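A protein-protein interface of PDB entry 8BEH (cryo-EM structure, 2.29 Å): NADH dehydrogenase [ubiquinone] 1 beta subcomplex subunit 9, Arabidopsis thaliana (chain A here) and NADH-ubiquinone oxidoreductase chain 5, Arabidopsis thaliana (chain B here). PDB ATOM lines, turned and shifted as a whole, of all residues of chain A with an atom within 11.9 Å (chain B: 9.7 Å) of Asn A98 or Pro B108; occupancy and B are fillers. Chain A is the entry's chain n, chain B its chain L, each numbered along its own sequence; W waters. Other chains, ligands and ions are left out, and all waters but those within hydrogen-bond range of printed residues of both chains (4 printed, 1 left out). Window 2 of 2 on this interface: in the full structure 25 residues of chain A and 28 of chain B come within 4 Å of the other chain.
Among the printed residues, merely in contact across the chains: Pro A99 with Thr B156 (3.4 Å), Arg A97 with Trp B154 (3.4 Å), Asn A98 with Pro B108 (3.5 Å), Asn A98 with Trp B154 (3.6 Å), Pro A87 with Asp B361 (3.7 Å), Cys A96 with Arg B157 (3.7 Å) and Ser A93 with Asp B361 (3.9 Å).
Of the 23 printed residues of chain B, 6 touch a printed residue of chain A. Printed residues of chain A that touch a printed residue of chain B: Pro A87, Gly A92, Ser A93, Lys A94, Phe A95, Cys A96, Arg A97, Asn A98 and Pro A99. Among the printed residues, Asp or Glu carboxylates within 4 Å of a Lys or Arg side-chain nitrogen of the other chain: Lys A94 with Asp B361 and Arg A97 with Asp B361.
Of the printed residues of chain B, Lys A94 touches Asp B361 (3.1 Å). Of the printed residues of chain B, Phe A95 touches Arg B157. Asn A98 touches three residues of chain B. Pro A99 touches one residue of chain B. Of the printed residues of chain A, Asp B107 touches Asn A98. Of chain A, only Asn A98 comes within 4 Å of Pro B108. No residue of chain A comes within 4 Å of His B109. No residue of chain A comes within 4 Å of Ser B110. Phe B153 touches none of the printed residues of chain A. Trp B154 touches just these residues of chain A: Arg A97 (3.4 Å) and Asn A98 (3.6 Å). Thr B156 touches just these residues of chain A: Cys A96 (2.7 Å) and Pro A99 (3.4 Å). Pro B249 touches none of the printed residues of chain A. The nearest residue of chain B that does not touch Asn A98 is Thr B156 (4.3 Å). The nearest residue of chain A that does not touch Pro B108 is Pro A99 (7.2 Å).
NH1 of Arg B157 sits at hydrogen-bond distance from O of Gly A92 (2.6 Å). The side-chain amide nitrogen (ND2) of Asn A98 sits at hydrogen-bond distance from the side-chain carboxylate (OD2) of Asp B107. The guanidinium group of Arg B157 lies within hydrogen-bond range of the backbone carbonyl oxygen of Phe A95. NH1 of Arg B157 lies within hydrogen-bond range of O of Ser A93. The side-chain carboxylate (OD2) of Asp B361 is in salt-bridge range of the side-chain amino group (NZ) of Lys A94, 3.1 Å away. OD1 of Asp B361 lies within salt-bridge range of NH1 of Arg A97 (3.3 Å). The side-chain hydroxyl of Thr B156 sits at hydrogen-bond distance from the backbone carbonyl oxygen of Cys A96, at 2.7 Å.
Water W3 lies within hydrogen-bond range of the side-chain hydroxyl of Thr B156 (2.6 Å) and the backbone NH of Asn A98 (3.2 Å). Water W2 lies within hydrogen-bond range of OD1 of Asp B107 (2.7 Å), OD1 of Asn A98 (2.8 Å) and ND1 of His B109 (2.8 Å). Water W1 lies within hydrogen-bond range of the side-chain carboxylate (OD1) of Asp B361 (2.8 Å) and the guanidinium group (NH2) of Arg A97 (3.2 Å). Water W4 bridges NH2 of Arg B157 and O of Gly A92.
The backbone carbonyl oxygen (O) of Pro A87 sits at hydrogen-bond distance from the backbone NH (N) of Phe A95, 3.1 Å away. The backbone NH (N) of Lys A94 lies within hydrogen-bond range of the backbone carbonyl oxygen (O) of Pro A87 (2.7 Å). The side-chain carboxylate of Asp B107 lies within hydrogen-bond range of the backbone NH of His B109, at 2.7 Å. The side-chain carboxylate (OD2) of Asp B107 lies within hydrogen-bond range of the indole nitrogen (NE1) of Trp B154, at 3.0 Å.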
ATOM      1  N   PRO A  87       3.110 -19.620 -23.477  1.00  0.00           N
ATOM      2  CA  PRO A  87       4.359 -20.382 -23.284  1.00  0.00           C
ATOM      3  C   PRO A  87       4.531 -20.999 -21.903  1.00  0.00           C
ATOM      4  O   PRO A  87       5.137 -22.071 -21.797  1.00  0.00           O
ATOM      5  CB  PRO A  87       5.444 -19.337 -23.577  1.00  0.00           C
ATOM      6  CG  PRO A  87       4.788 -18.355 -24.463  1.00  0.00           C
ATOM      7  CD  PRO A  87       3.361 -18.278 -24.030  1.00  0.00           C
ATOM      8  N   TRP A  88       4.026 -20.371 -20.844  1.00  0.00           N
ATOM      9  CA  TRP A  88       4.185 -20.921 -19.503  1.00  0.00           C
ATOM     10  C   TRP A  88       3.053 -21.858 -19.092  1.00  0.00           C
ATOM     11  O   TRP A  88       3.128 -22.456 -18.017  1.00  0.00           O
ATOM     12  CB  TRP A  88       4.326 -19.793 -18.473  1.00  0.00           C
ATOM     13  CG  TRP A  88       3.324 -18.701 -18.604  1.00  0.00           C
ATOM     14  CD1 TRP A  88       3.512 -17.487 -19.191  1.00  0.00           C
ATOM     15  CD2 TRP A  88       1.971 -18.716 -18.141  1.00  0.00           C
ATOM     16  NE1 TRP A  88       2.363 -16.743 -19.121  1.00  0.00           N
ATOM     17  CE2 TRP A  88       1.400 -17.476 -18.482  1.00  0.00           C
ATOM     18  CE3 TRP A  88       1.185 -19.660 -17.474  1.00  0.00           C
ATOM     19  CZ2 TRP A  88       0.080 -17.153 -18.178  1.00  0.00           C
ATOM     20  CZ3 TRP A  88      -0.126 -19.338 -17.175  1.00  0.00           C
ATOM     21  CH2 TRP A  88      -0.664 -18.097 -17.528  1.00  0.00           C
ATOM     22  N   GLY A  92       3.160 -25.577 -23.059  1.00  0.00           N
ATOM     23  CA  GLY A  92       3.788 -24.421 -23.656  1.00  0.00           C
ATOM     24  C   GLY A  92       5.287 -24.575 -23.819  1.00  0.00           C
ATOM     25  O   GLY A  92       5.921 -25.471 -23.269  1.00  0.00           O
ATOM     26  N   SER A  93       5.862 -23.654 -24.596  1.00  0.00           N
ATOM     27  CA  SER A  93       7.287 -23.715 -24.889  1.00  0.00           C
ATOM     28  C   SER A  93       8.150 -23.388 -23.675  1.00  0.00           C
ATOM     29  O   SER A  93       9.290 -23.853 -23.603  1.00  0.00           O
ATOM     30  CB  SER A  93       7.619 -22.774 -26.051  1.00  0.00           C
ATOM     31  OG  SER A  93       7.413 -21.421 -25.690  1.00  0.00           O
ATOM     32  N   LYS A  94       7.633 -22.615 -22.722  1.00  0.00           N
ATOM     33  CA  LYS A  94       8.349 -22.256 -21.503  1.00  0.00           C
ATOM     34  C   LYS A  94       7.941 -23.088 -20.289  1.00  0.00           C
ATOM     35  O   LYS A  94       8.434 -22.833 -19.187  1.00  0.00           O
ATOM     36  CB  LYS A  94       8.147 -20.775 -21.187  1.00  0.00           C
ATOM     37  CG  LYS A  94       9.424 -20.010 -20.958  1.00  0.00           C
ATOM     38  CD  LYS A  94       9.172 -18.819 -20.061  1.00  0.00           C
ATOM     39  CE  LYS A  94      10.368 -17.902 -20.007  1.00  0.00           C
ATOM     40  NZ  LYS A  94      10.006 -16.561 -19.482  1.00  0.00           N
ATOM     41  N   PHE A  95       7.060 -24.067 -20.459  1.00  0.00           N
ATOM     42  CA  PHE A  95       6.515 -24.800 -19.322  1.00  0.00           C
ATOM     43  C   PHE A  95       7.596 -25.646 -18.654  1.00  0.00           C
ATOM     44  O   PHE A  95       8.297 -26.415 -19.318  1.00  0.00           O
ATOM     45  CB  PHE A  95       5.347 -25.673 -19.782  1.00  0.00           C
ATOM     46  CG  PHE A  95       4.558 -26.283 -18.656  1.00  0.00           C
ATOM     47  CD1 PHE A  95       4.076 -25.498 -17.622  1.00  0.00           C
ATOM     48  CD2 PHE A  95       4.287 -27.641 -18.640  1.00  0.00           C
ATOM     49  CE1 PHE A  95       3.347 -26.057 -16.583  1.00  0.00           C
ATOM     50  CE2 PHE A  95       3.557 -28.206 -17.602  1.00  0.00           C
ATOM     51  CZ  PHE A  95       3.089 -27.412 -16.574  1.00  0.00           C
ATOM     52  N   CYS A  96       7.727 -25.491 -17.332  1.00  0.00           N
ATOM     53  CA  CYS A  96       8.676 -26.241 -16.499  1.00  0.00           C
ATOM     54  C   CYS A  96      10.138 -25.926 -16.824  1.00  0.00           C
ATOM     55  O   CYS A  96      11.010 -26.773 -16.624  1.00  0.00           O
ATOM     56  CB  CYS A  96       8.439 -27.752 -16.597  1.00  0.00           C
ATOM     57  SG  CYS A  96       6.737 -28.295 -16.328  1.00  0.00           S
ATOM     58  N   ARG A  97      10.346 -24.712 -17.319  1.00  0.00           N
ATOM     59  CA  ARG A  97      11.686 -24.167 -17.458  1.00  0.00           C
ATOM     60  C   ARG A  97      12.003 -23.360 -16.199  1.00  0.00           C
ATOM     61  O   ARG A  97      11.185 -22.597 -15.814  1.00  0.00           O
ATOM     62  CB  ARG A  97      11.787 -23.231 -18.656  1.00  0.00           C
ATOM     63  CG  ARG A  97      13.212 -22.796 -18.961  1.00  0.00           C
ATOM     64  CD  ARG A  97      13.309 -21.586 -19.866  1.00  0.00           C
ATOM     65  NE  ARG A  97      12.919 -21.904 -21.224  1.00  0.00           N
ATOM     66  CZ  ARG A  97      12.775 -21.030 -22.210  1.00  0.00           C
ATOM     67  NH1 ARG A  97      12.986 -19.745 -21.999  1.00  0.00           N
ATOM     68  NH2 ARG A  97      12.422 -21.454 -23.404  1.00  0.00           N
ATOM     69  N   ASN A  98      13.143 -23.594 -15.595  1.00  0.00           N
ATOM     70  CA  ASN A  98      13.579 -22.903 -14.354  1.00  0.00           C
ATOM     71  C   ASN A  98      12.440 -22.813 -13.312  1.00  0.00           C
ATOM     72  O   ASN A  98      12.185 -21.760 -12.845  1.00  0.00           O
ATOM     73  CB  ASN A  98      14.321 -21.613 -14.691  1.00  0.00           C
ATOM     74  CG  ASN A  98      15.473 -21.822 -15.645  1.00  0.00           C
ATOM     75  OD1 ASN A  98      16.200 -22.797 -15.534  1.00  0.00           O
ATOM     76  ND2 ASN A  98      15.638 -20.917 -16.585  1.00  0.00           N
ATOM     77  N   PRO A  99      11.784 -23.917 -12.943  1.00  0.00           N
ATOM     78  CA  PRO A  99      10.751 -23.847 -11.908  1.00  0.00           C
ATOM     79  C   PRO A  99      11.330 -23.477 -10.557  1.00  0.00           C
ATOM     80  O   PRO A  99      12.504 -23.719 -10.267  1.00  0.00           O
ATOM     81  CB  PRO A  99      10.178 -25.266 -11.890  1.00  0.00           C
ATOM     82  CG  PRO A  99      11.322 -26.121 -12.318  1.00  0.00           C
ATOM     83  CD  PRO A  99      12.122 -25.306 -13.297  1.00  0.00           C
ATOM     84  N   THR A 100      10.489 -22.875  -9.732  1.00  0.00           N
ATOM     85  CA  THR A 100      10.863 -22.668  -8.347  1.00  0.00           C
ATOM     86  C   THR A 100      11.031 -24.023  -7.667  1.00  0.00           C
ATOM     87  O   THR A 100      10.267 -24.955  -7.942  1.00  0.00           O
ATOM     88  CB  THR A 100       9.814 -21.828  -7.615  1.00  0.00           C
ATOM     89  OG1 THR A 100       9.711 -20.543  -8.239  1.00  0.00           O
ATOM     90  CG2 THR A 100      10.194 -21.644  -6.166  1.00  0.00           C
ATOM     91  N   PRO A 101      12.031 -24.177  -6.803  1.00  0.00           N
ATOM     92  CA  PRO A 101      12.249 -25.471  -6.170  1.00  0.00           C
ATOM     93  C   PRO A 101      11.088 -25.829  -5.265  1.00  0.00           C
ATOM     94  O   PRO A 101      10.421 -24.943  -4.698  1.00  0.00           O
ATOM     95  CB  PRO A 101      13.541 -25.260  -5.368  1.00  0.00           C
ATOM     96  CG  PRO A 101      14.142 -24.016  -5.879  1.00  0.00           C
ATOM     97  CD  PRO A 101      13.044 -23.180  -6.426  1.00  0.00           C
ATOM     98  N   PRO A 102      10.805 -27.116  -5.104  1.00  0.00           N
ATOM     99  CA  PRO A 102       9.784 -27.527  -4.136  1.00  0.00           C
ATOM    100  C   PRO A 102      10.213 -27.203  -2.715  1.00  0.00           C
ATOM    101  O   PRO A 102      11.403 -27.144  -2.395  1.00  0.00           O
ATOM    102  CB  PRO A 102       9.670 -29.041  -4.346  1.00  0.00           C
ATOM    103  CG  PRO A 102      10.936 -29.446  -5.019  1.00  0.00           C
ATOM    104  CD  PRO A 102      11.478 -28.255  -5.751  1.00  0.00           C
ATOM    105  N   GLY B  20      33.729 -23.506 -12.067  1.00  0.00           N
ATOM    106  CA  GLY B  20      32.693 -22.509 -12.233  1.00  0.00           C
ATOM    107  C   GLY B  20      32.202 -21.908 -10.934  1.00  0.00           C
ATOM    108  O   GLY B  20      31.696 -20.786 -10.938  1.00  0.00           O
ATOM    109  N   GLY B  24      31.745 -17.930 -11.223  1.00  0.00           N
ATOM    110  CA  GLY B  24      30.389 -17.526 -11.441  1.00  0.00           C
ATOM    111  C   GLY B  24      30.055 -17.312 -12.908  1.00  0.00           C
ATOM    112  O   GLY B  24      30.808 -17.645 -13.825  1.00  0.00           O
ATOM    113  N   SER B  25      28.880 -16.719 -13.099  1.00  0.00           N
ATOM    114  CA  SER B  25      28.373 -16.483 -14.446  1.00  0.00           C
ATOM    115  C   SER B  25      29.349 -15.646 -15.257  1.00  0.00           C
ATOM    116  O   SER B  25      29.743 -16.026 -16.368  1.00  0.00           O
ATOM    117  CB  SER B  25      27.017 -15.787 -14.367  1.00  0.00           C
ATOM    118  OG  SER B  25      26.131 -16.497 -13.534  1.00  0.00           O
ATOM    119  N   GLU B  26      29.774 -14.515 -14.694  1.00  0.00           N
ATOM    120  CA  GLU B  26      30.603 -13.569 -15.430  1.00  0.00           C
ATOM    121  C   GLU B  26      31.951 -14.168 -15.791  1.00  0.00           C
ATOM    122  O   GLU B  26      32.372 -14.112 -16.956  1.00  0.00           O
ATOM    123  CB  GLU B  26      30.782 -12.296 -14.609  1.00  0.00           C
ATOM    124  CG  GLU B  26      29.605 -11.372 -14.696  1.00  0.00           C
ATOM    125  CD  GLU B  26      28.521 -11.739 -13.732  1.00  0.00           C
ATOM    126  OE1 GLU B  26      28.749 -11.615 -12.516  1.00  0.00           O
ATOM    127  OE2 GLU B  26      27.446 -12.168 -14.197  1.00  0.00           O
ATOM    128  N   TYR B 103      22.326 -13.478 -23.862  1.00  0.00           N
ATOM    129  CA  TYR B 103      21.058 -14.179 -24.030  1.00  0.00           C
ATOM    130  C   TYR B 103      20.696 -15.010 -22.802  1.00  0.00           C
ATOM    131  O   TYR B 103      19.516 -15.134 -22.459  1.00  0.00           O
ATOM    132  CB  TYR B 103      21.110 -15.064 -25.274  1.00  0.00           C
ATOM    133  CG  TYR B 103      19.804 -15.755 -25.590  1.00  0.00           C
ATOM    134  CD1 TYR B 103      19.494 -16.994 -25.034  1.00  0.00           C
ATOM    135  CD2 TYR B 103      18.885 -15.178 -26.454  1.00  0.00           C
ATOM    136  CE1 TYR B 103      18.307 -17.626 -25.322  1.00  0.00           C
ATOM    137  CE2 TYR B 103      17.697 -15.807 -26.751  1.00  0.00           C
ATOM    138  CZ  TYR B 103      17.415 -17.032 -26.186  1.00  0.00           C
ATOM    139  OH  TYR B 103      16.229 -17.658 -26.482  1.00  0.00           O
ATOM    140  N   MET B 104      21.688 -15.606 -22.143  1.00  0.00           N
ATOM    141  CA  MET B 104      21.472 -16.437 -20.970  1.00  0.00           C
ATOM    142  C   MET B 104      21.769 -15.688 -19.679  1.00  0.00           C
ATOM    143  O   MET B 104      21.973 -16.314 -18.634  1.00  0.00           O
ATOM    144  CB  MET B 104      22.332 -17.699 -21.059  1.00  0.00           C
ATOM    145  CG  MET B 104      22.020 -18.594 -22.254  1.00  0.00           C
ATOM    146  SD  MET B 104      20.463 -19.491 -22.105  1.00  0.00           S
ATOM    147  CE  MET B 104      20.949 -20.833 -21.019  1.00  0.00           C
ATOM    148  N   SER B 105      21.789 -14.354 -19.734  1.00  0.00           N
ATOM    149  CA  SER B 105      22.232 -13.559 -18.594  1.00  0.00           C
ATOM    150  C   SER B 105      21.312 -13.718 -17.392  1.00  0.00           C
ATOM    151  O   SER B 105      21.771 -13.631 -16.249  1.00  0.00           O
ATOM    152  CB  SER B 105      22.336 -12.089 -18.996  1.00  0.00           C
ATOM    153  OG  SER B 105      21.065 -11.474 -19.001  1.00  0.00           O
ATOM    154  N   GLU B 106      20.024 -13.950 -17.619  1.00  0.00           N
ATOM    155  CA  GLU B 106      19.091 -14.170 -16.524  1.00  0.00           C
ATOM    156  C   GLU B 106      18.899 -15.645 -16.183  1.00  0.00           C
ATOM    157  O   GLU B 106      18.156 -15.955 -15.249  1.00  0.00           O
ATOM    158  CB  GLU B 106      17.733 -13.542 -16.847  1.00  0.00           C
ATOM    159  CG  GLU B 106      17.637 -12.057 -16.552  1.00  0.00           C
ATOM    160  CD  GLU B 106      18.609 -11.227 -17.361  1.00  0.00           C
ATOM    161  OE1 GLU B 106      18.583 -11.323 -18.606  1.00  0.00           O
ATOM    162  OE2 GLU B 106      19.406 -10.484 -16.752  1.00  0.00           O
ATOM    163  N   ASP B 107      19.533 -16.555 -16.914  1.00  0.00           N
ATOM    164  CA  ASP B 107      19.392 -17.970 -16.606  1.00  0.00           C
ATOM    165  C   ASP B 107      20.176 -18.321 -15.343  1.00  0.00           C
ATOM    166  O   ASP B 107      21.279 -17.811 -15.134  1.00  0.00           O
ATOM    167  CB  ASP B 107      19.866 -18.833 -17.776  1.00  0.00           C
ATOM    168  CG  ASP B 107      19.542 -20.308 -17.583  1.00  0.00           C
ATOM    169  OD1 ASP B 107      20.250 -20.983 -16.811  1.00  0.00           O
ATOM    170  OD2 ASP B 107      18.555 -20.782 -18.174  1.00  0.00           O
ATOM    171  N   PRO B 108      19.629 -19.184 -14.484  1.00  0.00           N
ATOM    172  CA  PRO B 108      20.350 -19.547 -13.254  1.00  0.00           C
ATOM    173  C   PRO B 108      21.644 -20.316 -13.486  1.00  0.00           C
ATOM    174  O   PRO B 108      22.537 -20.246 -12.637  1.00  0.00           O
ATOM    175  CB  PRO B 108      19.330 -20.399 -12.483  1.00  0.00           C
ATOM    176  CG  PRO B 108      18.017 -20.110 -13.102  1.00  0.00           C
ATOM    177  CD  PRO B 108      18.275 -19.761 -14.528  1.00  0.00           C
ATOM    178  N   HIS B 109      21.680 -21.086 -14.541  1.00  0.00           N
ATOM    179  CA  HIS B 109      22.825 -22.001 -14.739  1.00  0.00           C
ATOM    180  C   HIS B 109      23.768 -21.667 -15.925  1.00  0.00           C
ATOM    181  O   HIS B 109      24.271 -22.608 -16.534  1.00  0.00           O
ATOM    182  CB  HIS B 109      22.269 -23.427 -14.743  1.00  0.00           C
ATOM    183  CG  HIS B 109      21.481 -23.760 -13.534  1.00  0.00           C
ATOM    184  ND1 HIS B 109      20.116 -23.889 -13.571  1.00  0.00           N
ATOM    185  CD2 HIS B 109      21.847 -23.924 -12.251  1.00  0.00           C
ATOM    186  CE1 HIS B 109      19.680 -24.175 -12.377  1.00  0.00           C
ATOM    187  NE2 HIS B 109      20.711 -24.184 -11.557  1.00  0.00           N
ATOM    188  N   SER B 110      24.087 -20.423 -16.171  1.00  0.00           N
ATOM    189  CA  SER B 110      24.907 -20.057 -17.326  1.00  0.00           C
ATOM    190  C   SER B 110      26.296 -20.702 -17.358  1.00  0.00           C
ATOM    191  O   SER B 110      26.753 -21.034 -18.465  1.00  0.00           O
ATOM    192  CB  SER B 110      24.999 -18.528 -17.430  1.00  0.00           C
ATOM    193  OG  SER B 110      25.830 -17.967 -16.437  1.00  0.00           O
ATOM    194  N   PRO B 111      27.031 -20.870 -16.243  1.00  0.00           N
ATOM    195  CA  PRO B 111      28.357 -21.508 -16.359  1.00  0.00           C
ATOM    196  C   PRO B 111      28.327 -22.915 -16.942  1.00  0.00           C
ATOM    197  O   PRO B 111      29.177 -23.251 -17.779  1.00  0.00           O
ATOM    198  CB  PRO B 111      28.872 -21.500 -14.912  1.00  0.00           C
ATOM    199  CG  PRO B 111      28.135 -20.403 -14.261  1.00  0.00           C
ATOM    200  CD  PRO B 111      26.776 -20.430 -14.859  1.00  0.00           C
ATOM    201  N   ARG B 112      27.355 -23.742 -16.545  1.00  0.00           N
ATOM    202  CA  ARG B 112      27.237 -25.076 -17.127  1.00  0.00           C
ATOM    203  C   ARG B 112      26.941 -24.988 -18.619  1.00  0.00           C
ATOM    204  O   ARG B 112      27.470 -25.772 -19.416  1.00  0.00           O
ATOM    205  CB  ARG B 112      26.143 -25.875 -16.411  1.00  0.00           C
ATOM    206  CG  ARG B 112      26.187 -27.373 -16.687  1.00  0.00           C
ATOM    207  CD  ARG B 112      25.203 -28.168 -15.822  1.00  0.00           C
ATOM    208  NE  ARG B 112      23.940 -28.385 -16.513  1.00  0.00           N
ATOM    209  CZ  ARG B 112      22.805 -27.750 -16.253  1.00  0.00           C
ATOM    210  NH1 ARG B 112      22.700 -26.898 -15.249  1.00  0.00           N
ATOM    211  NH2 ARG B 112      21.748 -27.982 -17.021  1.00  0.00           N
ATOM    212  N   PHE B 113      26.096 -24.032 -19.005  1.00  0.00           N
ATOM    213  CA  PHE B 113      25.764 -23.828 -20.410  1.00  0.00           C
ATOM    214  C   PHE B 113      27.007 -23.477 -21.228  1.00  0.00           C
ATOM    215  O   PHE B 113      27.233 -24.040 -22.307  1.00  0.00           O
ATOM    216  CB  PHE B 113      24.704 -22.734 -20.519  1.00  0.00           C
ATOM    217  CG  PHE B 113      24.266 -22.449 -21.918  1.00  0.00           C
ATOM    218  CD1 PHE B 113      23.336 -23.261 -22.544  1.00  0.00           C
ATOM    219  CD2 PHE B 113      24.782 -21.365 -22.611  1.00  0.00           C
ATOM    220  CE1 PHE B 113      22.930 -22.997 -23.833  1.00  0.00           C
ATOM    221  CE2 PHE B 113      24.382 -21.099 -23.898  1.00  0.00           C
ATOM    222  CZ  PHE B 113      23.456 -21.914 -24.513  1.00  0.00           C
ATOM    223  N   HIS B 152      18.618 -30.996 -23.650  1.00  0.00           N
ATOM    224  CA  HIS B 152      17.910 -31.093 -22.380  1.00  0.00           C
ATOM    225  C   HIS B 152      18.587 -30.278 -21.277  1.00  0.00           C
ATOM    226  O   HIS B 152      18.522 -30.638 -20.098  1.00  0.00           O
ATOM    227  CB  HIS B 152      17.718 -32.567 -22.004  1.00  0.00           C
ATOM    228  CG  HIS B 152      18.820 -33.162 -21.183  1.00  0.00           C
ATOM    229  ND1 HIS B 152      18.664 -33.480 -19.851  1.00  0.00           N
ATOM    230  CD2 HIS B 152      20.082 -33.526 -21.511  1.00  0.00           C
ATOM    231  CE1 HIS B 152      19.787 -33.999 -19.388  1.00  0.00           C
ATOM    232  NE2 HIS B 152      20.663 -34.039 -20.376  1.00  0.00           N
ATOM    233  N   PHE B 153      19.192 -29.145 -21.654  1.00  0.00           N
ATOM    234  CA  PHE B 153      19.831 -28.256 -20.687  1.00  0.00           C
ATOM    235  C   PHE B 153      18.877 -27.852 -19.569  1.00  0.00           C
ATOM    236  O   PHE B 153      19.269 -27.795 -18.399  1.00  0.00           O
ATOM    237  CB  PHE B 153      20.368 -27.010 -21.394  1.00  0.00           C
ATOM    238  CG  PHE B 153      20.873 -25.954 -20.454  1.00  0.00           C
ATOM    239  CD1 PHE B 153      22.108 -26.086 -19.844  1.00  0.00           C
ATOM    240  CD2 PHE B 153      20.103 -24.841 -20.160  1.00  0.00           C
ATOM    241  CE1 PHE B 153      22.573 -25.125 -18.970  1.00  0.00           C
ATOM    242  CE2 PHE B 153      20.560 -23.877 -19.285  1.00  0.00           C
ATOM    243  CZ  PHE B 153      21.800 -24.019 -18.693  1.00  0.00           C
ATOM    244  N   TRP B 154      17.648 -27.505 -19.907  1.00  0.00           N
ATOM    245  CA  TRP B 154      16.533 -27.299 -18.942  1.00  0.00           C
ATOM    246  C   TRP B 154      15.994 -28.696 -18.528  1.00  0.00           C
ATOM    247  O   TRP B 154      14.958 -29.106 -19.031  1.00  0.00           O
ATOM    248  CB  TRP B 154      15.490 -26.359 -19.517  1.00  0.00           C
ATOM    249  CG  TRP B 154      15.996 -24.964 -19.708  1.00  0.00           C
ATOM    250  CD1 TRP B 154      16.659 -24.198 -18.795  1.00  0.00           C
ATOM    251  CD2 TRP B 154      15.890 -24.168 -20.900  1.00  0.00           C
ATOM    252  NE1 TRP B 154      16.941 -22.972 -19.324  1.00  0.00           N
ATOM    253  CE2 TRP B 154      16.485 -22.922 -20.613  1.00  0.00           C
ATOM    254  CE3 TRP B 154      15.336 -24.380 -22.165  1.00  0.00           C
ATOM    255  CZ2 TRP B 154      16.548 -21.898 -21.554  1.00  0.00           C
ATOM    256  CZ3 TRP B 154      15.401 -23.366 -23.097  1.00  0.00           C
ATOM    257  CH2 TRP B 154      16.001 -22.147 -22.792  1.00  0.00           C
ATOM    258  N   PHE B 155      16.708 -29.363 -17.663  1.00  0.00           N
ATOM    259  CA  PHE B 155      16.471 -30.787 -17.292  1.00  0.00           C
ATOM    260  C   PHE B 155      15.086 -31.078 -16.656  1.00  0.00           C
ATOM    261  O   PHE B 155      14.759 -32.198 -16.605  1.00  0.00           O
ATOM    262  CB  PHE B 155      17.676 -31.247 -16.474  1.00  0.00           C
ATOM    263  CG  PHE B 155      17.985 -30.446 -15.242  1.00  0.00           C
ATOM    264  CD1 PHE B 155      17.163 -30.508 -14.130  1.00  0.00           C
ATOM    265  CD2 PHE B 155      19.105 -29.635 -15.192  1.00  0.00           C
ATOM    266  CE1 PHE B 155      17.444 -29.753 -13.005  1.00  0.00           C
ATOM    267  CE2 PHE B 155      19.390 -28.886 -14.063  1.00  0.00           C
ATOM    268  CZ  PHE B 155      18.555 -28.947 -12.977  1.00  0.00           C
ATOM    269  N   THR B 156      14.377 -30.097 -16.186  1.00  0.00           N
ATOM    270  CA  THR B 156      13.042 -30.248 -15.549  1.00  0.00           C
ATOM    271  C   THR B 156      11.944 -30.389 -16.611  1.00  0.00           C
ATOM    272  O   THR B 156      10.890 -30.746 -16.258  1.00  0.00           O
ATOM    273  CB  THR B 156      12.882 -29.124 -14.502  1.00  0.00           C
ATOM    274  OG1 THR B 156      12.969 -27.914 -15.251  1.00  0.00           O
ATOM    275  CG2 THR B 156      13.918 -29.134 -13.405  1.00  0.00           C
ATOM    276  N   ARG B 157      12.259 -30.064 -17.865  1.00  0.00           N
ATOM    277  CA  ARG B 157      11.238 -30.071 -18.903  1.00  0.00           C
ATOM    278  C   ARG B 157      11.155 -31.452 -19.540  1.00  0.00           C
ATOM    279  O   ARG B 157      12.149 -31.955 -20.070  1.00  0.00           O
ATOM    280  CB  ARG B 157      11.559 -29.016 -19.958  1.00  0.00           C
ATOM    281  CG  ARG B 157      10.381 -28.554 -20.743  1.00  0.00           C
ATOM    282  CD  ARG B 157      10.717 -27.318 -21.555  1.00  0.00           C
ATOM    283  NE  ARG B 157      10.179 -27.443 -22.901  1.00  0.00           N
ATOM    284  CZ  ARG B 157       8.929 -27.161 -23.229  1.00  0.00           C
ATOM    285  NH1 ARG B 157       8.072 -26.690 -22.340  1.00  0.00           N
ATOM    286  NH2 ARG B 157       8.526 -27.367 -24.479  1.00  0.00           N
ATOM    287  N   PRO B 249      18.037 -24.199 -25.849  1.00  0.00           N
ATOM    288  CA  PRO B 249      18.094 -22.736 -25.961  1.00  0.00           C
ATOM    289  C   PRO B 249      18.561 -22.304 -27.346  1.00  0.00           C
ATOM    290  O   PRO B 249      19.337 -22.995 -28.007  1.00  0.00           O
ATOM    291  CB  PRO B 249      19.102 -22.340 -24.877  1.00  0.00           C
ATOM    292  CG  PRO B 249      19.067 -23.485 -23.902  1.00  0.00           C
ATOM    293  CD  PRO B 249      18.863 -24.704 -24.742  1.00  0.00           C
ATOM    294  N   ASP B 361       9.528 -14.476 -24.636  1.00  0.00           N
ATOM    295  CA  ASP B 361       9.607 -15.884 -25.011  1.00  0.00           C
ATOM    296  C   ASP B 361       8.384 -16.380 -25.771  1.00  0.00           C
ATOM    297  O   ASP B 361       8.110 -17.581 -25.782  1.00  0.00           O
ATOM    298  CB  ASP B 361       9.859 -16.772 -23.787  1.00  0.00           C
ATOM    299  CG  ASP B 361      11.219 -16.532 -23.178  1.00  0.00           C
ATOM    300  OD1 ASP B 361      12.212 -17.076 -23.702  1.00  0.00           O
ATOM    301  OD2 ASP B 361      11.295 -15.785 -22.186  1.00  0.00           O
HETATM  302  O   HOH W   1      11.573 -19.172 -25.492  1.00  0.00           O
HETATM  303  O   HOH W   2      18.908 -23.208 -15.987  1.00  0.00           O
HETATM  304  O   HOH W   3      14.708 -26.293 -16.291  1.00  0.00           O
HETATM  305  O   HOH W   4       5.756 -28.062 -24.811  1.00  0.00           O
